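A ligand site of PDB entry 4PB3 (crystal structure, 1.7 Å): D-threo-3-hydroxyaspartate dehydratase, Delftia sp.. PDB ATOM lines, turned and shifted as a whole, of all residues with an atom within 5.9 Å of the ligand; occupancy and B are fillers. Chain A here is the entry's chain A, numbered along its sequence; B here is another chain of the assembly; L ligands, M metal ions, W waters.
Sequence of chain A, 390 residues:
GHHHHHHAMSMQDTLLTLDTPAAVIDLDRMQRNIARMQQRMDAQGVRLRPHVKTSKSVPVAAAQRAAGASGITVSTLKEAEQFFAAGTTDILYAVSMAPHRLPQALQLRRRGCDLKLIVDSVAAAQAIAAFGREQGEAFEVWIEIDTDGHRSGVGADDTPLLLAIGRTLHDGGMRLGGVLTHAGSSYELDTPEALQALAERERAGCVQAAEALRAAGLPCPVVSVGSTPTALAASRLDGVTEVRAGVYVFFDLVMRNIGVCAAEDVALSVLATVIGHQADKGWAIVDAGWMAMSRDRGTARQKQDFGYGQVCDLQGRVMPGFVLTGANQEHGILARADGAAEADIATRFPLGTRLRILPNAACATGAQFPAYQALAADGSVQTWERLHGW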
ATOM      1  N   HIS A  51      -9.794  14.850   4.868  1.00  0.00           N
ATOM      2  CA  HIS A  51      -9.896  13.906   5.949  1.00  0.00           C
ATOM      3  C   HIS A  51      -9.258  12.615   5.436  1.00  0.00           C
ATOM      4  O   HIS A  51      -9.795  11.938   4.541  1.00  0.00           O
ATOM      5  CB  HIS A  51     -11.346  13.639   6.321  1.00  0.00           C
ATOM      6  CG  HIS A  51     -11.464  13.145   7.704  1.00  0.00           C
ATOM      7  ND1 HIS A  51     -10.625  12.170   8.158  1.00  0.00           N
ATOM      8  CD2 HIS A  51     -12.178  13.604   8.787  1.00  0.00           C
ATOM      9  CE1 HIS A  51     -10.874  11.978   9.491  1.00  0.00           C
ATOM     10  NE2 HIS A  51     -11.807  12.849   9.862  1.00  0.00           N
ATOM     11  N   LYS A  53      -9.060   9.859   6.878  1.00  0.00           N
ATOM     12  CA  LYS A  53      -9.609   8.545   7.441  1.00  0.00           C
ATOM     13  C   LYS A  53     -10.048   7.628   6.239  1.00  0.00           C
ATOM     14  O   LYS A  53     -10.173   6.434   6.425  1.00  0.00           O
ATOM     15  CB  LYS A  53     -10.744   8.721   8.443  1.00  0.00           C
ATOM     16  CG  LYS A  53     -12.073   9.159   7.761  1.00  0.00           C
ATOM     17  CD  LYS A  53     -13.095   9.268   8.936  1.00  0.00           C
ATOM     18  CE  LYS A  53     -14.446   9.476   8.303  1.00  0.00           C
ATOM     19  NZ  LYS A  53     -15.073  10.750   8.790  1.00  0.00           N
ATOM     20  N   THR A  54     -10.285   8.232   5.055  1.00  0.00           N
ATOM     21  CA  THR A  54     -10.656   7.380   3.889  1.00  0.00           C
ATOM     22  C   THR A  54      -9.542   6.485   3.443  1.00  0.00           C
ATOM     23  O   THR A  54      -9.819   5.320   3.148  1.00  0.00           O
ATOM     24  CB  THR A  54     -11.055   8.334   2.706  1.00  0.00           C
ATOM     25  OG1 THR A  54     -12.279   8.978   3.111  1.00  0.00           O
ATOM     26  CG2 THR A  54     -11.386   7.470   1.491  1.00  0.00           C
ATOM     27  N   THR A  73      -7.195  16.226   8.382  1.00  0.00           N
ATOM     28  CA  THR A  73      -8.029  15.871   9.492  1.00  0.00           C
ATOM     29  C   THR A  73      -7.792  14.375   9.657  1.00  0.00           C
ATOM     30  O   THR A  73      -7.707  13.647   8.676  1.00  0.00           O
ATOM     31  CB  THR A  73      -9.528  16.043   9.141  1.00  0.00           C
ATOM     32  OG1 THR A  73      -9.710  17.391   8.615  1.00  0.00           O
ATOM     33  CG2 THR A  73     -10.391  15.933  10.406  1.00  0.00           C
ATOM     34  N   ALA A  94     -10.355  15.024  14.688  1.00  0.00           N
ATOM     35  CA  ALA A  94     -11.761  15.440  14.743  1.00  0.00           C
ATOM     36  C   ALA A  94     -12.671  14.396  15.301  1.00  0.00           C
ATOM     37  O   ALA A  94     -13.710  14.032  14.680  1.00  0.00           O
ATOM     38  CB  ALA A  94     -12.184  15.938  13.329  1.00  0.00           C
ATOM     39  N   GLU A 144     -16.896  21.581  18.725  1.00  0.00           N
ATOM     40  CA  GLU A 144     -17.685  20.938  17.662  1.00  0.00           C
ATOM     41  C   GLU A 144     -19.143  21.391  17.861  1.00  0.00           C
ATOM     42  O   GLU A 144     -19.701  21.414  19.004  1.00  0.00           O
ATOM     43  CB  GLU A 144     -17.618  19.426  17.808  1.00  0.00           C
ATOM     44  CG  GLU A 144     -18.355  18.719  16.666  1.00  0.00           C
ATOM     45  CD  GLU A 144     -18.068  17.218  16.597  1.00  0.00           C
ATOM     46  OE1 GLU A 144     -18.371  16.692  15.520  1.00  0.00           O
ATOM     47  OE2 GLU A 144     -17.672  16.617  17.639  1.00  0.00           O
ATOM     48  N   ARG A 151     -24.618  13.533  15.048  1.00  0.00           N
ATOM     49  CA  ARG A 151     -23.558  12.836  15.853  1.00  0.00           C
ATOM     50  C   ARG A 151     -23.188  13.707  17.059  1.00  0.00           C
ATOM     51  O   ARG A 151     -24.109  14.031  17.788  1.00  0.00           O
ATOM     52  CB  ARG A 151     -22.319  12.559  14.998  1.00  0.00           C
ATOM     53  CG  ARG A 151     -21.580  11.283  15.409  1.00  0.00           C
ATOM     54  CD  ARG A 151     -20.637  10.879  14.298  1.00  0.00           C
ATOM     55  NE  ARG A 151     -19.617  11.936  14.052  1.00  0.00           N
ATOM     56  CZ  ARG A 151     -18.889  11.941  12.913  1.00  0.00           C
ATOM     57  NH1 ARG A 151     -19.207  11.000  11.943  1.00  0.00           N
ATOM     58  NH2 ARG A 151     -17.862  12.804  12.769  1.00  0.00           N
ATOM     59  N   LEU A 180     -16.059  23.764  14.562  1.00  0.00           N
ATOM     60  CA  LEU A 180     -16.161  22.922  13.396  1.00  0.00           C
ATOM     61  C   LEU A 180     -17.504  22.199  13.444  1.00  0.00           C
ATOM     62  O   LEU A 180     -18.076  22.057  14.521  1.00  0.00           O
ATOM     63  CB  LEU A 180     -15.039  21.839  13.285  1.00  0.00           C
ATOM     64  CG  LEU A 180     -15.099  20.581  14.220  1.00  0.00           C
ATOM     65  CD1 LEU A 180     -14.209  19.496  13.632  1.00  0.00           C
ATOM     66  CD2 LEU A 180     -14.752  21.025  15.677  1.00  0.00           C
ATOM     67  N   THR A 181     -17.981  21.755  12.272  1.00  0.00           N
ATOM     68  CA  THR A 181     -19.180  20.917  12.263  1.00  0.00           C
ATOM     69  C   THR A 181     -19.006  19.940  11.134  1.00  0.00           C
ATOM     70  O   THR A 181     -18.340  20.249  10.109  1.00  0.00           O
ATOM     71  CB  THR A 181     -20.485  21.795  12.091  1.00  0.00           C
ATOM     72  OG1 THR A 181     -21.623  20.942  12.234  1.00  0.00           O
ATOM     73  CG2 THR A 181     -20.454  22.467  10.672  1.00  0.00           C
ATOM     74  N   HIS A 182     -19.723  18.796  11.213  1.00  0.00           N
ATOM     75  CA  HIS A 182     -19.791  17.846  10.088  1.00  0.00           C
ATOM     76  C   HIS A 182     -21.207  17.439   9.878  1.00  0.00           C
ATOM     77  O   HIS A 182     -21.843  16.854  10.787  1.00  0.00           O
ATOM     78  CB  HIS A 182     -18.943  16.624  10.500  1.00  0.00           C
ATOM     79  CG  HIS A 182     -19.091  15.449   9.608  1.00  0.00           C
ATOM     80  ND1 HIS A 182     -18.633  15.419   8.323  1.00  0.00           N
ATOM     81  CD2 HIS A 182     -19.611  14.132   9.900  1.00  0.00           C
ATOM     82  CE1 HIS A 182     -18.805  14.117   7.802  1.00  0.00           C
ATOM     83  NE2 HIS A 182     -19.394  13.349   8.769  1.00  0.00           N
ATOM     84  N   SER A 186     -26.069  14.449   5.513  1.00  0.00           N
ATOM     85  CA  SER A 186     -26.048  14.576   4.009  1.00  0.00           C
ATOM     86  C   SER A 186     -26.059  13.233   3.387  1.00  0.00           C
ATOM     87  O   SER A 186     -26.565  13.027   2.250  1.00  0.00           O
ATOM     88  CB  SER A 186     -24.786  15.304   3.497  1.00  0.00           C
ATOM     89  OG  SER A 186     -23.586  14.558   3.788  1.00  0.00           O
ATOM     90  N   TYR A 187     -25.611  12.285   4.143  1.00  0.00           N
ATOM     91  CA  TYR A 187     -25.620  10.889   3.555  1.00  0.00           C
ATOM     92  C   TYR A 187     -26.989  10.304   3.331  1.00  0.00           C
ATOM     93  O   TYR A 187     -27.074   9.322   2.537  1.00  0.00           O
ATOM     94  CB  TYR A 187     -24.750   9.923   4.435  1.00  0.00           C
ATOM     95  CG  TYR A 187     -23.288  10.134   4.184  1.00  0.00           C
ATOM     96  CD1 TYR A 187     -22.643  11.348   4.417  1.00  0.00           C
ATOM     97  CD2 TYR A 187     -22.550   9.093   3.648  1.00  0.00           C
ATOM     98  CE1 TYR A 187     -21.238  11.508   4.230  1.00  0.00           C
ATOM     99  CE2 TYR A 187     -21.173   9.201   3.460  1.00  0.00           C
ATOM    100  CZ  TYR A 187     -20.539  10.441   3.675  1.00  0.00           C
ATOM    101  OH  TYR A 187     -19.163  10.544   3.380  1.00  0.00           O
ATOM    102  N   GLY A 226     -17.941  20.564   6.845  1.00  0.00           N
ATOM    103  CA  GLY A 226     -17.923  19.744   5.655  1.00  0.00           C
ATOM    104  C   GLY A 226     -18.196  18.249   5.812  1.00  0.00           C
ATOM    105  O   GLY A 226     -17.930  17.628   6.906  1.00  0.00           O
ATOM    106  N   SER A 227     -18.669  17.715   4.722  1.00  0.00           N
ATOM    107  CA  SER A 227     -18.765  16.259   4.433  1.00  0.00           C
ATOM    108  C   SER A 227     -18.490  16.281   2.928  1.00  0.00           C
ATOM    109  O   SER A 227     -18.572  17.359   2.315  1.00  0.00           O
ATOM    110  CB  SER A 227     -20.164  15.701   4.740  1.00  0.00           C
ATOM    111  OG  SER A 227     -21.182  16.352   3.962  1.00  0.00           O
ATOM    112  N   THR A 228     -18.239  15.146   2.296  1.00  0.00           N
ATOM    113  CA  THR A 228     -17.996  15.245   0.853  1.00  0.00           C
ATOM    114  C   THR A 228     -19.259  15.774   0.139  1.00  0.00           C
ATOM    115  O   THR A 228     -19.115  16.678  -0.745  1.00  0.00           O
ATOM    116  CB  THR A 228     -17.496  13.882   0.262  1.00  0.00           C
ATOM    117  OG1 THR A 228     -16.091  13.805   0.538  1.00  0.00           O
ATOM    118  CG2 THR A 228     -17.716  13.774  -1.278  1.00  0.00           C
ATOM    119  N   PRO A 229     -20.480  15.259   0.448  1.00  0.00           N
ATOM    120  CA  PRO A 229     -21.652  15.785  -0.258  1.00  0.00           C
ATOM    121  C   PRO A 229     -21.888  17.279  -0.032  1.00  0.00           C
ATOM    122  O   PRO A 229     -22.179  18.023  -1.040  1.00  0.00           O
ATOM    123  CB  PRO A 229     -22.840  14.946   0.253  1.00  0.00           C
ATOM    124  CG  PRO A 229     -22.159  13.633   0.676  1.00  0.00           C
ATOM    125  CD  PRO A 229     -20.812  14.056   1.282  1.00  0.00           C
ATOM    126  N   ARG A 244     -13.687  20.435   5.259  1.00  0.00           N
ATOM    127  CA  ARG A 244     -13.085  19.080   5.472  1.00  0.00           C
ATOM    128  C   ARG A 244     -13.870  18.082   4.651  1.00  0.00           C
ATOM    129  O   ARG A 244     -15.079  18.039   4.732  1.00  0.00           O
ATOM    130  CB  ARG A 244     -13.184  18.625   6.937  1.00  0.00           C
ATOM    131  CG  ARG A 244     -12.512  19.720   7.889  1.00  0.00           C
ATOM    132  CD  ARG A 244     -12.559  19.212   9.375  1.00  0.00           C
ATOM    133  NE  ARG A 244     -13.814  18.560   9.629  1.00  0.00           N
ATOM    134  CZ  ARG A 244     -14.999  19.190   9.729  1.00  0.00           C
ATOM    135  NH1 ARG A 244     -15.061  20.567   9.820  1.00  0.00           N
ATOM    136  NH2 ARG A 244     -16.142  18.469   9.721  1.00  0.00           N
ATOM    137  N   ALA A 245     -13.172  17.298   3.834  1.00  0.00           N
ATOM    138  CA  ALA A 245     -13.825  16.242   3.027  1.00  0.00           C
ATOM    139  C   ALA A 245     -12.764  15.162   2.831  1.00  0.00           C
ATOM    140  O   ALA A 245     -11.576  15.487   2.730  1.00  0.00           O
ATOM    141  CB  ALA A 245     -14.250  16.797   1.607  1.00  0.00           C
ATOM    142  N   GLY A 246     -13.228  13.920   2.723  1.00  0.00           N
ATOM    143  CA  GLY A 246     -12.274  12.771   2.592  1.00  0.00           C
ATOM    144  C   GLY A 246     -12.709  11.756   1.516  1.00  0.00           C
ATOM    145  O   GLY A 246     -11.844  11.335   0.763  1.00  0.00           O
ATOM    146  N   VAL A 247     -13.974  11.334   1.543  1.00  0.00           N
ATOM    147  CA  VAL A 247     -14.282  10.152   0.702  1.00  0.00           C
ATOM    148  C   VAL A 247     -14.189  10.500  -0.757  1.00  0.00           C
ATOM    149  O   VAL A 247     -13.936   9.592  -1.581  1.00  0.00           O
ATOM    150  CB  VAL A 247     -15.638   9.527   1.095  1.00  0.00           C
ATOM    151  CG1 VAL A 247     -16.835  10.443   0.669  1.00  0.00           C
ATOM    152  CG2 VAL A 247     -15.767   8.127   0.457  1.00  0.00           C
ATOM    153  N   TYR A 248     -14.279  11.798  -1.084  1.00  0.00           N
ATOM    154  CA  TYR A 248     -14.238  12.218  -2.523  1.00  0.00           C
ATOM    155  C   TYR A 248     -12.933  11.783  -3.174  1.00  0.00           C
ATOM    156  O   TYR A 248     -12.881  11.653  -4.397  1.00  0.00           O
ATOM    157  CB  TYR A 248     -14.338  13.798  -2.513  1.00  0.00           C
ATOM    158  CG  TYR A 248     -12.958  14.379  -2.203  1.00  0.00           C
ATOM    159  CD1 TYR A 248     -12.551  14.566  -0.836  1.00  0.00           C
ATOM    160  CD2 TYR A 248     -12.022  14.687  -3.264  1.00  0.00           C
ATOM    161  CE1 TYR A 248     -11.258  15.047  -0.564  1.00  0.00           C
ATOM    162  CE2 TYR A 248     -10.750  15.198  -2.967  1.00  0.00           C
ATOM    163  CZ  TYR A 248     -10.371  15.334  -1.601  1.00  0.00           C
ATOM    164  OH  TYR A 248      -9.170  15.880  -1.351  1.00  0.00           O
ATOM    165  N   MET A 255     -21.784   7.445  -2.541  1.00  0.00           N
ATOM    166  CA  MET A 255     -21.697   8.819  -3.119  1.00  0.00           C
ATOM    167  C   MET A 255     -22.363   8.876  -4.451  1.00  0.00           C
ATOM    168  O   MET A 255     -23.004   9.920  -4.756  1.00  0.00           O
ATOM    169  CB  MET A 255     -20.232   9.245  -3.239  1.00  0.00           C
ATOM    170  CG  MET A 255     -19.485   9.428  -1.899  1.00  0.00           C
ATOM    171  SD  MET A 255     -20.158  10.884  -1.014  1.00  0.00           S
ATOM    172  CE  MET A 255     -20.699   9.927   0.389  1.00  0.00           C
ATOM    173  N   CYS A 363     -14.410   4.141   2.562  1.00  0.00           N
ATOM    174  CA  CYS A 363     -13.707   4.174   3.863  1.00  0.00           C
ATOM    175  C   CYS A 363     -13.712   2.769   4.501  1.00  0.00           C
ATOM    176  O   CYS A 363     -12.725   2.366   5.171  1.00  0.00           O
ATOM    177  CB  CYS A 363     -14.487   5.021   4.871  1.00  0.00           C
ATOM    178  SG  CYS A 363     -14.266   6.838   4.496  1.00  0.00           S
ATOM    179  N   GLN B 329     -17.739   6.049  11.913  1.00  0.00           N
ATOM    180  CA  GLN B 329     -16.479   5.268  11.717  1.00  0.00           C
ATOM    181  C   GLN B 329     -15.737   5.074  13.066  1.00  0.00           C
ATOM    182  O   GLN B 329     -15.353   3.925  13.411  1.00  0.00           O
ATOM    183  CB  GLN B 329     -15.580   6.039  10.729  1.00  0.00           C
ATOM    184  CG  GLN B 329     -14.397   5.153  10.275  1.00  0.00           C
ATOM    185  CD  GLN B 329     -13.769   5.664   8.989  1.00  0.00           C
ATOM    186  OE1 GLN B 329     -14.458   6.084   8.019  1.00  0.00           O
ATOM    187  NE2 GLN B 329     -12.416   5.605   8.899  1.00  0.00           N
ATOM    188  N   HIS B 331     -17.070   6.650  16.051  1.00  0.00           N
ATOM    189  CA  HIS B 331     -17.991   7.018  17.095  1.00  0.00           C
ATOM    190  C   HIS B 331     -19.074   6.000  17.094  1.00  0.00           C
ATOM    191  O   HIS B 331     -19.679   5.789  16.057  1.00  0.00           O
ATOM    192  CB  HIS B 331     -18.783   8.347  16.663  1.00  0.00           C
ATOM    193  CG  HIS B 331     -17.980   9.593  16.458  1.00  0.00           C
ATOM    194  ND1 HIS B 331     -17.221   9.820  15.378  1.00  0.00           N
ATOM    195  CD2 HIS B 331     -17.942  10.756  17.230  1.00  0.00           C
ATOM    196  CE1 HIS B 331     -16.618  11.076  15.492  1.00  0.00           C
ATOM    197  NE2 HIS B 331     -17.087  11.654  16.597  1.00  0.00           N
HETATM  198  N1  LIG L   1     -15.393  15.807   9.158  1.00  0.00           N
HETATM  199  C1  LIG L   1     -15.545  14.859  10.098  1.00  0.00           C
HETATM  200  C2  LIG L   1     -15.693  15.193  11.560  1.00  0.00           C
HETATM  201  C3  LIG L   1     -15.564  13.481   9.665  1.00  0.00           C
HETATM  202  O1  LIG L   1     -15.685  12.530  10.626  1.00  0.00           O
HETATM  203  C4  LIG L   1     -15.413  13.084   8.267  1.00  0.00           C
HETATM  204  C5  LIG L   1     -15.272  11.703   7.764  1.00  0.00           C
HETATM  205  C6  LIG L   1     -15.327  14.198   7.308  1.00  0.00           C
HETATM  206  C7  LIG L   1     -15.275  15.511   7.841  1.00  0.00           C
HETATM  207  C8  LIG L   1     -15.151  13.916   5.796  1.00  0.00           C
HETATM  208  O2  LIG L   1     -16.524  13.677   5.310  1.00  0.00           O
HETATM  209  P1  LIG L   1     -16.637  12.623   4.104  1.00  0.00           P
HETATM  210  O3  LIG L   1     -15.696  13.067   3.113  1.00  0.00           O
HETATM  211  O4  LIG L   1     -18.105  12.778   3.663  1.00  0.00           O
HETATM  212  O5  LIG L   1     -16.293  11.216   4.566  1.00  0.00           O
HETATM  213 MG    MG M   1     -17.574   7.601   5.673  1.00  0.00          MG
HETATM  214  O   HOH W   1     -14.813  10.413  11.480  1.00  0.00           O
HETATM  215  O   HOH W   2     -13.585  10.820   4.917  1.00  0.00           O
HETATM  216  O   HOH W   3     -13.044  12.409  12.405  1.00  0.00           O
HETATM  217  O   HOH W   4     -17.237   9.581   6.263  1.00  0.00           O
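The side-chain hydroxyl (OG) of Ser 227 sits at hydrogen-bond distance from the side-chain hydroxyl (OG) of Ser 186 (3.0 Å).
The guanidinium group (NE) of Arg 151 lies close to a ring nitrogen (ND1) of His 331 of chain B, at 3.5 Å.
The backbone carbonyl oxygen of Thr 73 sits at hydrogen-bond distance from a ring nitrogen (ND1) of His 51 (3.3 Å).
The backbone NH of His 51 lies within hydrogen-bond range of the backbone carbonyl oxygen of Ala 245.
The backbone NH (N) of Val 247 lies within hydrogen-bond range of the side-chain hydroxyl (OG1) of Thr 54 (3.3 Å).
O of Lys 53 is in hydrogen-bond range of NE2 of Gln 329 of chain B.
OG1 of Thr 54 lies close to O of Gly 246, at 3.4 Å.
The guanidinium group of Arg 244 sits at hydrogen-bond distance from the backbone carbonyl oxygen of Thr 181 (2.9 Å).
A nitrogen (N1) of the ligand is in hydrogen-bond range of the guanidinium group (NH2) of Arg 244.
A nitrogen (N1) of the ligand sits at hydrogen-bond distance from a ring nitrogen (ND1) of His 182, 3.4 Å away.
The guanidinium group of Arg 151 lies within hydrogen-bond range of an oxygen (O1) of the ligand, 3.1 Å away.
O4 of the ligand lies within hydrogen-bond range of N of Thr 228.
The side-chain hydroxyl (OG1) of Thr 228 lies within hydrogen-bond range of an oxygen (O3) of the ligand (2.7 Å).
The side-chain hydroxyl of Tyr 187 is in hydrogen-bond range of an oxygen (O4) of the ligand (2.5 Å).
O3 of the ligand is in hydrogen-bond range of N of Val 247.
The backbone NH (N) of Gly 246 is in hydrogen-bond range of an oxygen (O3) of the ligand.
NZ of Lys 53 is covalently linked to C5 of the ligand.
Water W1 bridges O1 of the ligand (2.4 Å) and NZ of Lys 53 (2.7 Å).
Water W2 lies within hydrogen-bond range of O5 of the ligand (2.8 Å), OG1 of Thr 54 (2.9 Å) and N of Val 247 (3.4 Å).
Water W3 lies within hydrogen-bond range of a ring nitrogen (NE2) of His 51, the backbone carbonyl oxygen of Ala 94 and an oxygen (O1) of the ligand.
Residues that only touch the ligand: His 51, Ala 94, Gly 226, Ser 227, Pro 229 and Ala 245.
The nearest printed residue that does not touch the ligand is Tyr 248 (4.6 Å).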
